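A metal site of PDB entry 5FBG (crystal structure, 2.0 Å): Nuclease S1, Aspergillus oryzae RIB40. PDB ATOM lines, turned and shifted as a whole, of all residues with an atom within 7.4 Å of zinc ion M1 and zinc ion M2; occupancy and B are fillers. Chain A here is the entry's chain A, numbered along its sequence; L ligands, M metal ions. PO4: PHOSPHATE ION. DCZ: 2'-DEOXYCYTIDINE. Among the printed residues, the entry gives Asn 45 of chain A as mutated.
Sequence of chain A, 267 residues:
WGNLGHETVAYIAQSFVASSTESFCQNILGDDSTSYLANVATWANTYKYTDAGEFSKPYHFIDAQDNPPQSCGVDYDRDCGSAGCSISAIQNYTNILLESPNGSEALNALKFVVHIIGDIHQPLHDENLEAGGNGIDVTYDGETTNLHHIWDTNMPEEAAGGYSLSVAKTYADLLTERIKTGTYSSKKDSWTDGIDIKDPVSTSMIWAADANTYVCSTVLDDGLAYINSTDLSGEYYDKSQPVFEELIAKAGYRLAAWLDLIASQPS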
ATOM      1  N   TRP A   1      11.866 -16.258  -4.083  1.00  0.00           N
ATOM      2  CA  TRP A   1      11.995 -14.922  -4.569  1.00  0.00           C
ATOM      3  C   TRP A   1      12.252 -13.974  -3.402  1.00  0.00           C
ATOM      4  O   TRP A   1      11.859 -14.255  -2.264  1.00  0.00           O
ATOM      5  CB  TRP A   1      10.775 -14.433  -5.343  1.00  0.00           C
ATOM      6  CG  TRP A   1      10.333 -15.378  -6.429  1.00  0.00           C
ATOM      7  CD1 TRP A   1       9.308 -16.230  -6.369  1.00  0.00           C
ATOM      8  CD2 TRP A   1      10.940 -15.548  -7.740  1.00  0.00           C
ATOM      9  NE1 TRP A   1       9.170 -16.884  -7.581  1.00  0.00           N
ATOM     10  CE2 TRP A   1      10.174 -16.472  -8.431  1.00  0.00           C
ATOM     11  CE3 TRP A   1      12.045 -14.963  -8.379  1.00  0.00           C
ATOM     12  CZ2 TRP A   1      10.508 -16.908  -9.740  1.00  0.00           C
ATOM     13  CZ3 TRP A   1      12.358 -15.363  -9.681  1.00  0.00           C
ATOM     14  CH2 TRP A   1      11.597 -16.333 -10.352  1.00  0.00           C
ATOM     15  N   GLY A   2      12.795 -12.810  -3.755  1.00  0.00           N
ATOM     16  CA  GLY A   2      12.812 -11.665  -2.858  1.00  0.00           C
ATOM     17  C   GLY A   2      11.425 -10.993  -2.844  1.00  0.00           C
ATOM     18  O   GLY A   2      10.445 -11.500  -3.407  1.00  0.00           O
ATOM     19  N   ASN A   3      11.351  -9.867  -2.165  1.00  0.00           N
ATOM     20  CA  ASN A   3      10.038  -9.194  -1.935  1.00  0.00           C
ATOM     21  C   ASN A   3       9.359  -8.785  -3.217  1.00  0.00           C
ATOM     22  O   ASN A   3       8.197  -9.018  -3.367  1.00  0.00           O
ATOM     23  CB  ASN A   3      10.219  -7.998  -1.016  1.00  0.00           C
ATOM     24  CG  ASN A   3      10.572  -8.423   0.408  1.00  0.00           C
ATOM     25  OD1 ASN A   3      10.617  -9.632   0.752  1.00  0.00           O
ATOM     26  ND2 ASN A   3      10.821  -7.463   1.234  1.00  0.00           N
ATOM     27  N   GLY A   5       9.589 -10.084  -6.239  1.00  0.00           N
ATOM     28  CA  GLY A   5       9.023 -11.275  -6.902  1.00  0.00           C
ATOM     29  C   GLY A   5       7.754 -11.756  -6.258  1.00  0.00           C
ATOM     30  O   GLY A   5       6.772 -12.005  -6.931  1.00  0.00           O
ATOM     31  N   HIS A   6       7.758 -11.904  -4.936  1.00  0.00           N
ATOM     32  CA  HIS A   6       6.579 -12.354  -4.222  1.00  0.00           C
ATOM     33  C   HIS A   6       5.386 -11.406  -4.384  1.00  0.00           C
ATOM     34  O   HIS A   6       4.263 -11.869  -4.533  1.00  0.00           O
ATOM     35  CB  HIS A   6       6.830 -12.605  -2.725  1.00  0.00           C
ATOM     36  CG  HIS A   6       7.615 -13.847  -2.480  1.00  0.00           C
ATOM     37  ND1 HIS A   6       7.070 -15.086  -2.607  1.00  0.00           N
ATOM     38  CD2 HIS A   6       8.936 -14.030  -2.201  1.00  0.00           C
ATOM     39  CE1 HIS A   6       8.014 -16.004  -2.453  1.00  0.00           C
ATOM     40  NE2 HIS A   6       9.153 -15.391  -2.217  1.00  0.00           N
ATOM     41  N   ALA A  41       2.535 -11.253   1.104  1.00  0.00           N
ATOM     42  CA  ALA A  41       3.255 -12.199   0.234  1.00  0.00           C
ATOM     43  C   ALA A  41       4.674 -12.547   0.734  1.00  0.00           C
ATOM     44  O   ALA A  41       5.265 -13.527   0.254  1.00  0.00           O
ATOM     45  CB  ALA A  41       3.337 -11.663  -1.195  1.00  0.00           C
ATOM     46  N   THR A  42       5.220 -11.719   1.628  1.00  0.00           N
ATOM     47  CA  THR A  42       6.515 -11.985   2.198  1.00  0.00           C
ATOM     48  C   THR A  42       6.444 -12.514   3.622  1.00  0.00           C
ATOM     49  O   THR A  42       7.481 -12.873   4.199  1.00  0.00           O
ATOM     50  CB  THR A  42       7.449 -10.761   2.172  1.00  0.00           C
ATOM     51  OG1 THR A  42       7.014  -9.781   3.133  1.00  0.00           O
ATOM     52  CG2 THR A  42       7.463 -10.137   0.800  1.00  0.00           C
ATOM     53  N   ALA A  44       5.750 -15.254   5.107  1.00  0.00           N
ATOM     54  CA  ALA A  44       6.331 -16.546   5.468  1.00  0.00           C
ATOM     55  C   ALA A  44       7.829 -16.419   5.710  1.00  0.00           C
ATOM     56  O   ALA A  44       8.373 -17.123   6.589  1.00  0.00           O
ATOM     57  CB  ALA A  44       6.028 -17.586   4.450  1.00  0.00           C
ATOM     58  N   ASN A  45       8.473 -15.529   4.932  1.00  0.00           N
ATOM     59  CA  ASN A  45       9.849 -15.228   5.172  1.00  0.00           C
ATOM     60  C   ASN A  45      10.063 -14.578   6.524  1.00  0.00           C
ATOM     61  O   ASN A  45      10.908 -15.002   7.294  1.00  0.00           O
ATOM     62  CB  ASN A  45      10.486 -14.390   4.059  1.00  0.00           C
ATOM     63  CG  ASN A  45      10.836 -15.215   2.838  1.00  0.00           C
ATOM     64  OD1 ASN A  45      10.791 -16.428   2.876  1.00  0.00           O
ATOM     65  ND2 ASN A  45      11.125 -14.548   1.765  1.00  0.00           N
ATOM     66  N   LYS A  48       9.580 -17.248   9.371  1.00  0.00           N
ATOM     67  CA  LYS A  48      10.601 -18.314   9.515  1.00  0.00           C
ATOM     68  C   LYS A  48      11.818 -17.866  10.400  1.00  0.00           C
ATOM     69  O   LYS A  48      12.531 -18.732  10.937  1.00  0.00           O
ATOM     70  CB  LYS A  48      11.073 -18.850   8.174  1.00  0.00           C
ATOM     71  CG  LYS A  48      12.067 -17.946   7.460  1.00  0.00           C
ATOM     72  CD  LYS A  48      12.226 -18.440   6.026  1.00  0.00           C
ATOM     73  CE  LYS A  48      13.223 -17.724   5.154  1.00  0.00           C
ATOM     74  NZ  LYS A  48      13.157 -18.206   3.717  1.00  0.00           N
ATOM     75  N   LYS A  57      11.164 -22.972   8.135  1.00  0.00           N
ATOM     76  CA  LYS A  57      12.193 -22.693   7.154  1.00  0.00           C
ATOM     77  C   LYS A  57      12.273 -23.669   5.949  1.00  0.00           C
ATOM     78  O   LYS A  57      12.484 -23.236   4.845  1.00  0.00           O
ATOM     79  CB  LYS A  57      13.604 -22.619   7.805  1.00  0.00           C
ATOM     80  CG  LYS A  57      13.886 -21.284   8.493  1.00  0.00           C
ATOM     81  CD  LYS A  57      15.221 -21.303   9.252  1.00  0.00           C
ATOM     82  CE  LYS A  57      15.373 -19.963   9.948  1.00  0.00           C
ATOM     83  NZ  LYS A  57      16.689 -19.849  10.634  1.00  0.00           N
ATOM     84  N   TYR A  59      10.033 -25.251   4.498  1.00  0.00           N
ATOM     85  CA  TYR A  59       8.788 -25.219   3.713  1.00  0.00           C
ATOM     86  C   TYR A  59       8.895 -24.338   2.486  1.00  0.00           C
ATOM     87  O   TYR A  59       7.996 -24.280   1.700  1.00  0.00           O
ATOM     88  CB  TYR A  59       7.592 -24.776   4.581  1.00  0.00           C
ATOM     89  CG  TYR A  59       7.237 -25.596   5.809  1.00  0.00           C
ATOM     90  CD1 TYR A  59       7.836 -26.823   6.095  1.00  0.00           C
ATOM     91  CD2 TYR A  59       6.238 -25.151   6.661  1.00  0.00           C
ATOM     92  CE1 TYR A  59       7.451 -27.583   7.201  1.00  0.00           C
ATOM     93  CE2 TYR A  59       5.831 -25.883   7.746  1.00  0.00           C
ATOM     94  CZ  TYR A  59       6.429 -27.097   8.027  1.00  0.00           C
ATOM     95  OH  TYR A  59       5.997 -27.790   9.134  1.00  0.00           O
ATOM     96  N   HIS A  60      10.019 -23.655   2.321  1.00  0.00           N
ATOM     97  CA  HIS A  60      10.201 -22.740   1.211  1.00  0.00           C
ATOM     98  C   HIS A  60      10.790 -23.341  -0.045  1.00  0.00           C
ATOM     99  O   HIS A  60      10.880 -22.643  -1.117  1.00  0.00           O
ATOM    100  CB  HIS A  60      11.091 -21.559   1.690  1.00  0.00           C
ATOM    101  CG  HIS A  60      10.403 -20.730   2.718  1.00  0.00           C
ATOM    102  ND1 HIS A  60      10.026 -19.420   2.484  1.00  0.00           N
ATOM    103  CD2 HIS A  60       9.877 -21.078   3.924  1.00  0.00           C
ATOM    104  CE1 HIS A  60       9.371 -18.971   3.537  1.00  0.00           C
ATOM    105  NE2 HIS A  60       9.224 -19.965   4.408  1.00  0.00           N
ATOM    106  N   PHE A  61      11.202 -24.611   0.040  1.00  0.00           N
ATOM    107  CA  PHE A  61      11.919 -25.253  -1.079  1.00  0.00           C
ATOM    108  C   PHE A  61      11.744 -26.750  -1.039  1.00  0.00           C
ATOM    109  O   PHE A  61      11.202 -27.354  -0.097  1.00  0.00           O
ATOM    110  CB  PHE A  61      13.411 -24.815  -1.081  1.00  0.00           C
ATOM    111  CG  PHE A  61      14.094 -25.077   0.224  1.00  0.00           C
ATOM    112  CD1 PHE A  61      14.604 -26.345   0.518  1.00  0.00           C
ATOM    113  CD2 PHE A  61      14.219 -24.052   1.169  1.00  0.00           C
ATOM    114  CE1 PHE A  61      15.207 -26.593   1.723  1.00  0.00           C
ATOM    115  CE2 PHE A  61      14.835 -24.280   2.389  1.00  0.00           C
ATOM    116  CZ  PHE A  61      15.322 -25.543   2.682  1.00  0.00           C
ATOM    117  N   HIS A 115       2.807 -17.267  -0.452  1.00  0.00           N
ATOM    118  CA  HIS A 115       4.248 -17.168  -0.536  1.00  0.00           C
ATOM    119  C   HIS A 115       4.868 -18.404  -1.248  1.00  0.00           C
ATOM    120  O   HIS A 115       5.703 -18.264  -2.121  1.00  0.00           O
ATOM    121  CB  HIS A 115       4.867 -17.023   0.866  1.00  0.00           C
ATOM    122  CG  HIS A 115       6.356 -16.878   0.842  1.00  0.00           C
ATOM    123  ND1 HIS A 115       6.972 -15.675   0.681  1.00  0.00           N
ATOM    124  CD2 HIS A 115       7.351 -17.799   0.930  1.00  0.00           C
ATOM    125  CE1 HIS A 115       8.284 -15.836   0.685  1.00  0.00           C
ATOM    126  NE2 HIS A 115       8.537 -17.116   0.847  1.00  0.00           N
ATOM    127  N   ILE A 116       4.429 -19.583  -0.841  1.00  0.00           N
ATOM    128  CA  ILE A 116       5.101 -20.821  -1.223  1.00  0.00           C
ATOM    129  C   ILE A 116       4.805 -21.176  -2.698  1.00  0.00           C
ATOM    130  O   ILE A 116       5.695 -21.585  -3.388  1.00  0.00           O
ATOM    131  CB  ILE A 116       4.786 -21.961  -0.255  1.00  0.00           C
ATOM    132  CG1 ILE A 116       5.392 -21.652   1.106  1.00  0.00           C
ATOM    133  CG2 ILE A 116       5.356 -23.261  -0.789  1.00  0.00           C
ATOM    134  CD1 ILE A 116       4.904 -22.601   2.195  1.00  0.00           C
ATOM    135  N   GLY A 118       4.587 -18.988  -4.873  1.00  0.00           N
ATOM    136  CA  GLY A 118       5.619 -18.135  -5.495  1.00  0.00           C
ATOM    137  C   GLY A 118       6.973 -18.861  -5.501  1.00  0.00           C
ATOM    138  O   GLY A 118       7.645 -18.967  -6.544  1.00  0.00           O
ATOM    139  N   ASP A 119       7.408 -19.281  -4.323  1.00  0.00           N
ATOM    140  CA  ASP A 119       8.779 -19.852  -4.143  1.00  0.00           C
ATOM    141  C   ASP A 119       9.022 -21.113  -5.002  1.00  0.00           C
ATOM    142  O   ASP A 119      10.090 -21.257  -5.589  1.00  0.00           O
ATOM    143  CB  ASP A 119       9.022 -20.203  -2.688  1.00  0.00           C
ATOM    144  CG  ASP A 119       9.744 -19.157  -1.902  1.00  0.00           C
ATOM    145  OD1 ASP A 119      10.207 -18.119  -2.468  1.00  0.00           O
ATOM    146  OD2 ASP A 119       9.790 -19.381  -0.671  1.00  0.00           O
ATOM    147  N   ILE A 120       7.987 -21.956  -5.131  1.00  0.00           N
ATOM    148  CA  ILE A 120       8.034 -23.143  -5.997  1.00  0.00           C
ATOM    149  C   ILE A 120       8.483 -22.807  -7.402  1.00  0.00           C
ATOM    150  O   ILE A 120       9.177 -23.609  -8.076  1.00  0.00           O
ATOM    151  CB  ILE A 120       6.704 -23.927  -5.965  1.00  0.00           C
ATOM    152  CG1 ILE A 120       6.536 -24.592  -4.584  1.00  0.00           C
ATOM    153  CG2 ILE A 120       6.633 -24.970  -7.116  1.00  0.00           C
ATOM    154  CD1 ILE A 120       5.132 -25.092  -4.332  1.00  0.00           C
ATOM    155  N   GLN A 122      10.524 -20.439  -8.415  1.00  0.00           N
ATOM    156  CA  GLN A 122      11.888 -19.975  -8.504  1.00  0.00           C
ATOM    157  C   GLN A 122      12.732 -21.265  -8.640  1.00  0.00           C
ATOM    158  O   GLN A 122      12.753 -22.048  -7.702  1.00  0.00           O
ATOM    159  CB  GLN A 122      12.280 -19.190  -7.241  1.00  0.00           C
ATOM    160  CG  GLN A 122      13.390 -18.174  -7.421  1.00  0.00           C
ATOM    161  CD  GLN A 122      14.824 -18.802  -7.520  1.00  0.00           C
ATOM    162  OE1 GLN A 122      15.099 -19.563  -8.460  1.00  0.00           O
ATOM    163  NE2 GLN A 122      15.683 -18.463  -6.604  1.00  0.00           N
ATOM    164  N   HIS A 125      14.723 -22.934  -5.892  1.00  0.00           N
ATOM    165  CA  HIS A 125      13.920 -23.512  -4.769  1.00  0.00           C
ATOM    166  C   HIS A 125      13.485 -24.925  -5.028  1.00  0.00           C
ATOM    167  O   HIS A 125      12.748 -25.507  -4.233  1.00  0.00           O
ATOM    168  CB  HIS A 125      12.673 -22.616  -4.565  1.00  0.00           C
ATOM    169  CG  HIS A 125      12.967 -21.372  -3.777  1.00  0.00           C
ATOM    170  ND1 HIS A 125      12.498 -21.205  -2.494  1.00  0.00           N
ATOM    171  CD2 HIS A 125      13.710 -20.294  -4.059  1.00  0.00           C
ATOM    172  CE1 HIS A 125      12.960 -20.070  -2.015  1.00  0.00           C
ATOM    173  NE2 HIS A 125      13.674 -19.491  -2.946  1.00  0.00           N
ATOM    174  N   HIS A 148      21.746 -18.058  -5.893  1.00  0.00           N
ATOM    175  CA  HIS A 148      20.380 -18.092  -5.431  1.00  0.00           C
ATOM    176  C   HIS A 148      19.841 -16.637  -5.333  1.00  0.00           C
ATOM    177  O   HIS A 148      18.729 -16.319  -5.805  1.00  0.00           O
ATOM    178  CB  HIS A 148      20.271 -18.741  -4.079  1.00  0.00           C
ATOM    179  CG  HIS A 148      18.861 -18.914  -3.617  1.00  0.00           C
ATOM    180  ND1 HIS A 148      18.202 -20.127  -3.698  1.00  0.00           N
ATOM    181  CD2 HIS A 148      17.957 -18.027  -3.126  1.00  0.00           C
ATOM    182  CE1 HIS A 148      16.950 -19.973  -3.253  1.00  0.00           C
ATOM    183  NE2 HIS A 148      16.808 -18.726  -2.867  1.00  0.00           N
ATOM    184  N   ASP A 152      16.570 -14.714  -6.965  1.00  0.00           N
ATOM    185  CA  ASP A 152      15.519 -14.243  -6.068  1.00  0.00           C
ATOM    186  C   ASP A 152      15.258 -12.725  -6.270  1.00  0.00           C
ATOM    187  O   ASP A 152      14.111 -12.293  -6.313  1.00  0.00           O
ATOM    188  CB  ASP A 152      15.889 -14.469  -4.597  1.00  0.00           C
ATOM    189  CG  ASP A 152      15.313 -15.739  -3.981  1.00  0.00           C
ATOM    190  OD1 ASP A 152      14.712 -16.598  -4.628  1.00  0.00           O
ATOM    191  OD2 ASP A 152      15.557 -15.911  -2.770  1.00  0.00           O
HETATM  192  P   PO4 L   1      12.927 -17.069   0.131  1.00  0.00           P
HETATM  193  O1  PO4 L   1      11.693 -16.451  -0.478  1.00  0.00           O
HETATM  194  O2  PO4 L   1      12.494 -18.323   0.899  1.00  0.00           O
HETATM  195  O3  PO4 L   1      13.978 -17.386  -0.883  1.00  0.00           O
HETATM  196  O4  PO4 L   1      13.667 -16.264   1.173  1.00  0.00           O
HETATM  197  N1  DCZ L   2      16.871 -21.752   0.159  1.00  0.00           N
HETATM  198  C2  DCZ L   2      16.526 -22.675  -0.837  1.00  0.00           C
HETATM  199  N3  DCZ L   2      17.053 -23.943  -0.781  1.00  0.00           N
HETATM  200  C4  DCZ L   2      17.842 -24.303   0.238  1.00  0.00           C
HETATM  201  C5  DCZ L   2      18.216 -23.366   1.271  1.00  0.00           C
HETATM  202  C6  DCZ L   2      17.733 -22.114   1.188  1.00  0.00           C
HETATM  203  O2  DCZ L   2      15.703 -22.342  -1.686  1.00  0.00           O
HETATM  204  N4  DCZ L   2      18.269 -25.549   0.292  1.00  0.00           N
HETATM  205  C1' DCZ L   2      16.231 -20.421   0.151  1.00  0.00           C
HETATM  206  C2' DCZ L   2      15.458 -20.076   1.429  1.00  0.00           C
HETATM  207  C3' DCZ L   2      16.398 -19.111   2.185  1.00  0.00           C
HETATM  208  C4' DCZ L   2      17.136 -18.445   1.037  1.00  0.00           C
HETATM  209  O4' DCZ L   2      17.256 -19.464   0.015  1.00  0.00           O
HETATM  210  O3' DCZ L   2      15.796 -18.042   2.924  1.00  0.00           O
HETATM  211  C5' DCZ L   2      18.513 -17.877   1.365  1.00  0.00           C
HETATM  212  O5' DCZ L   2      18.884 -17.020   0.271  1.00  0.00           O
HETATM  213 ZN    ZN M   1      10.411 -18.111   0.940  1.00  0.00          ZN
HETATM  214 ZN    ZN M   2      10.973 -16.233  -2.129  1.00  0.00          ZN
HETATM  215 ZN    ZN M   3      14.939 -17.847  -2.422  1.00  0.00          ZN
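NZ of Lys 48 sits at hydrogen-bond distance from O3' of DCZ L2 (2.8 Å). A ring nitrogen (ND1) of His 125 is in hydrogen-bond range of an oxygen (O2) of DCZ L2, 3.5 Å away. NE2 of His 148 lies close to O4' of DCZ L2.
ND1 of His 6 sits close to ND1 of His 115 (3.3 Å). O of His 60 lies within hydrogen-bond range of ND1 of His 125. The backbone carbonyl oxygen of Ala 41 lies within hydrogen-bond range of a ring nitrogen (ND1) of His 115 (2.8 Å). The indole nitrogen (NE1) of Trp 1 lies within hydrogen-bond range of the backbone carbonyl oxygen (O) of Gly 118 (2.8 Å). The side-chain amide oxygen of Asn 45 lies close to the side-chain amino group of Lys 48, at 3.1 Å.
NZ of Lys 48 touches zinc ion M1, 3.9 Å away. Within 4 Å of zinc ion M1: Asn 45, Lys 48, His 60, His 115 and Asp 119.
Zinc ion M1 is bound by a ring nitrogen (ND1) of His 60 (2.1 Å), an oxygen (O2) of PO4 L1 (2.1 Å), a ring nitrogen (NE2) of His 115 (2.1 Å), the side-chain carboxylate of Asp 119 (2.1 Å), an oxygen (O1) of PO4 L1 (2.5 Å) and the side-chain amide oxygen of Asn 45 (2.6 Å). Zinc ion M1 has six donor atoms within binding distance.
Zinc ion M2 is bound by O1 of PO4 L1, NE2 of His 6, OD1 of Asp 119, N of Trp 1 and O of Trp 1. Zinc ion M2 has five donor atoms within binding distance.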
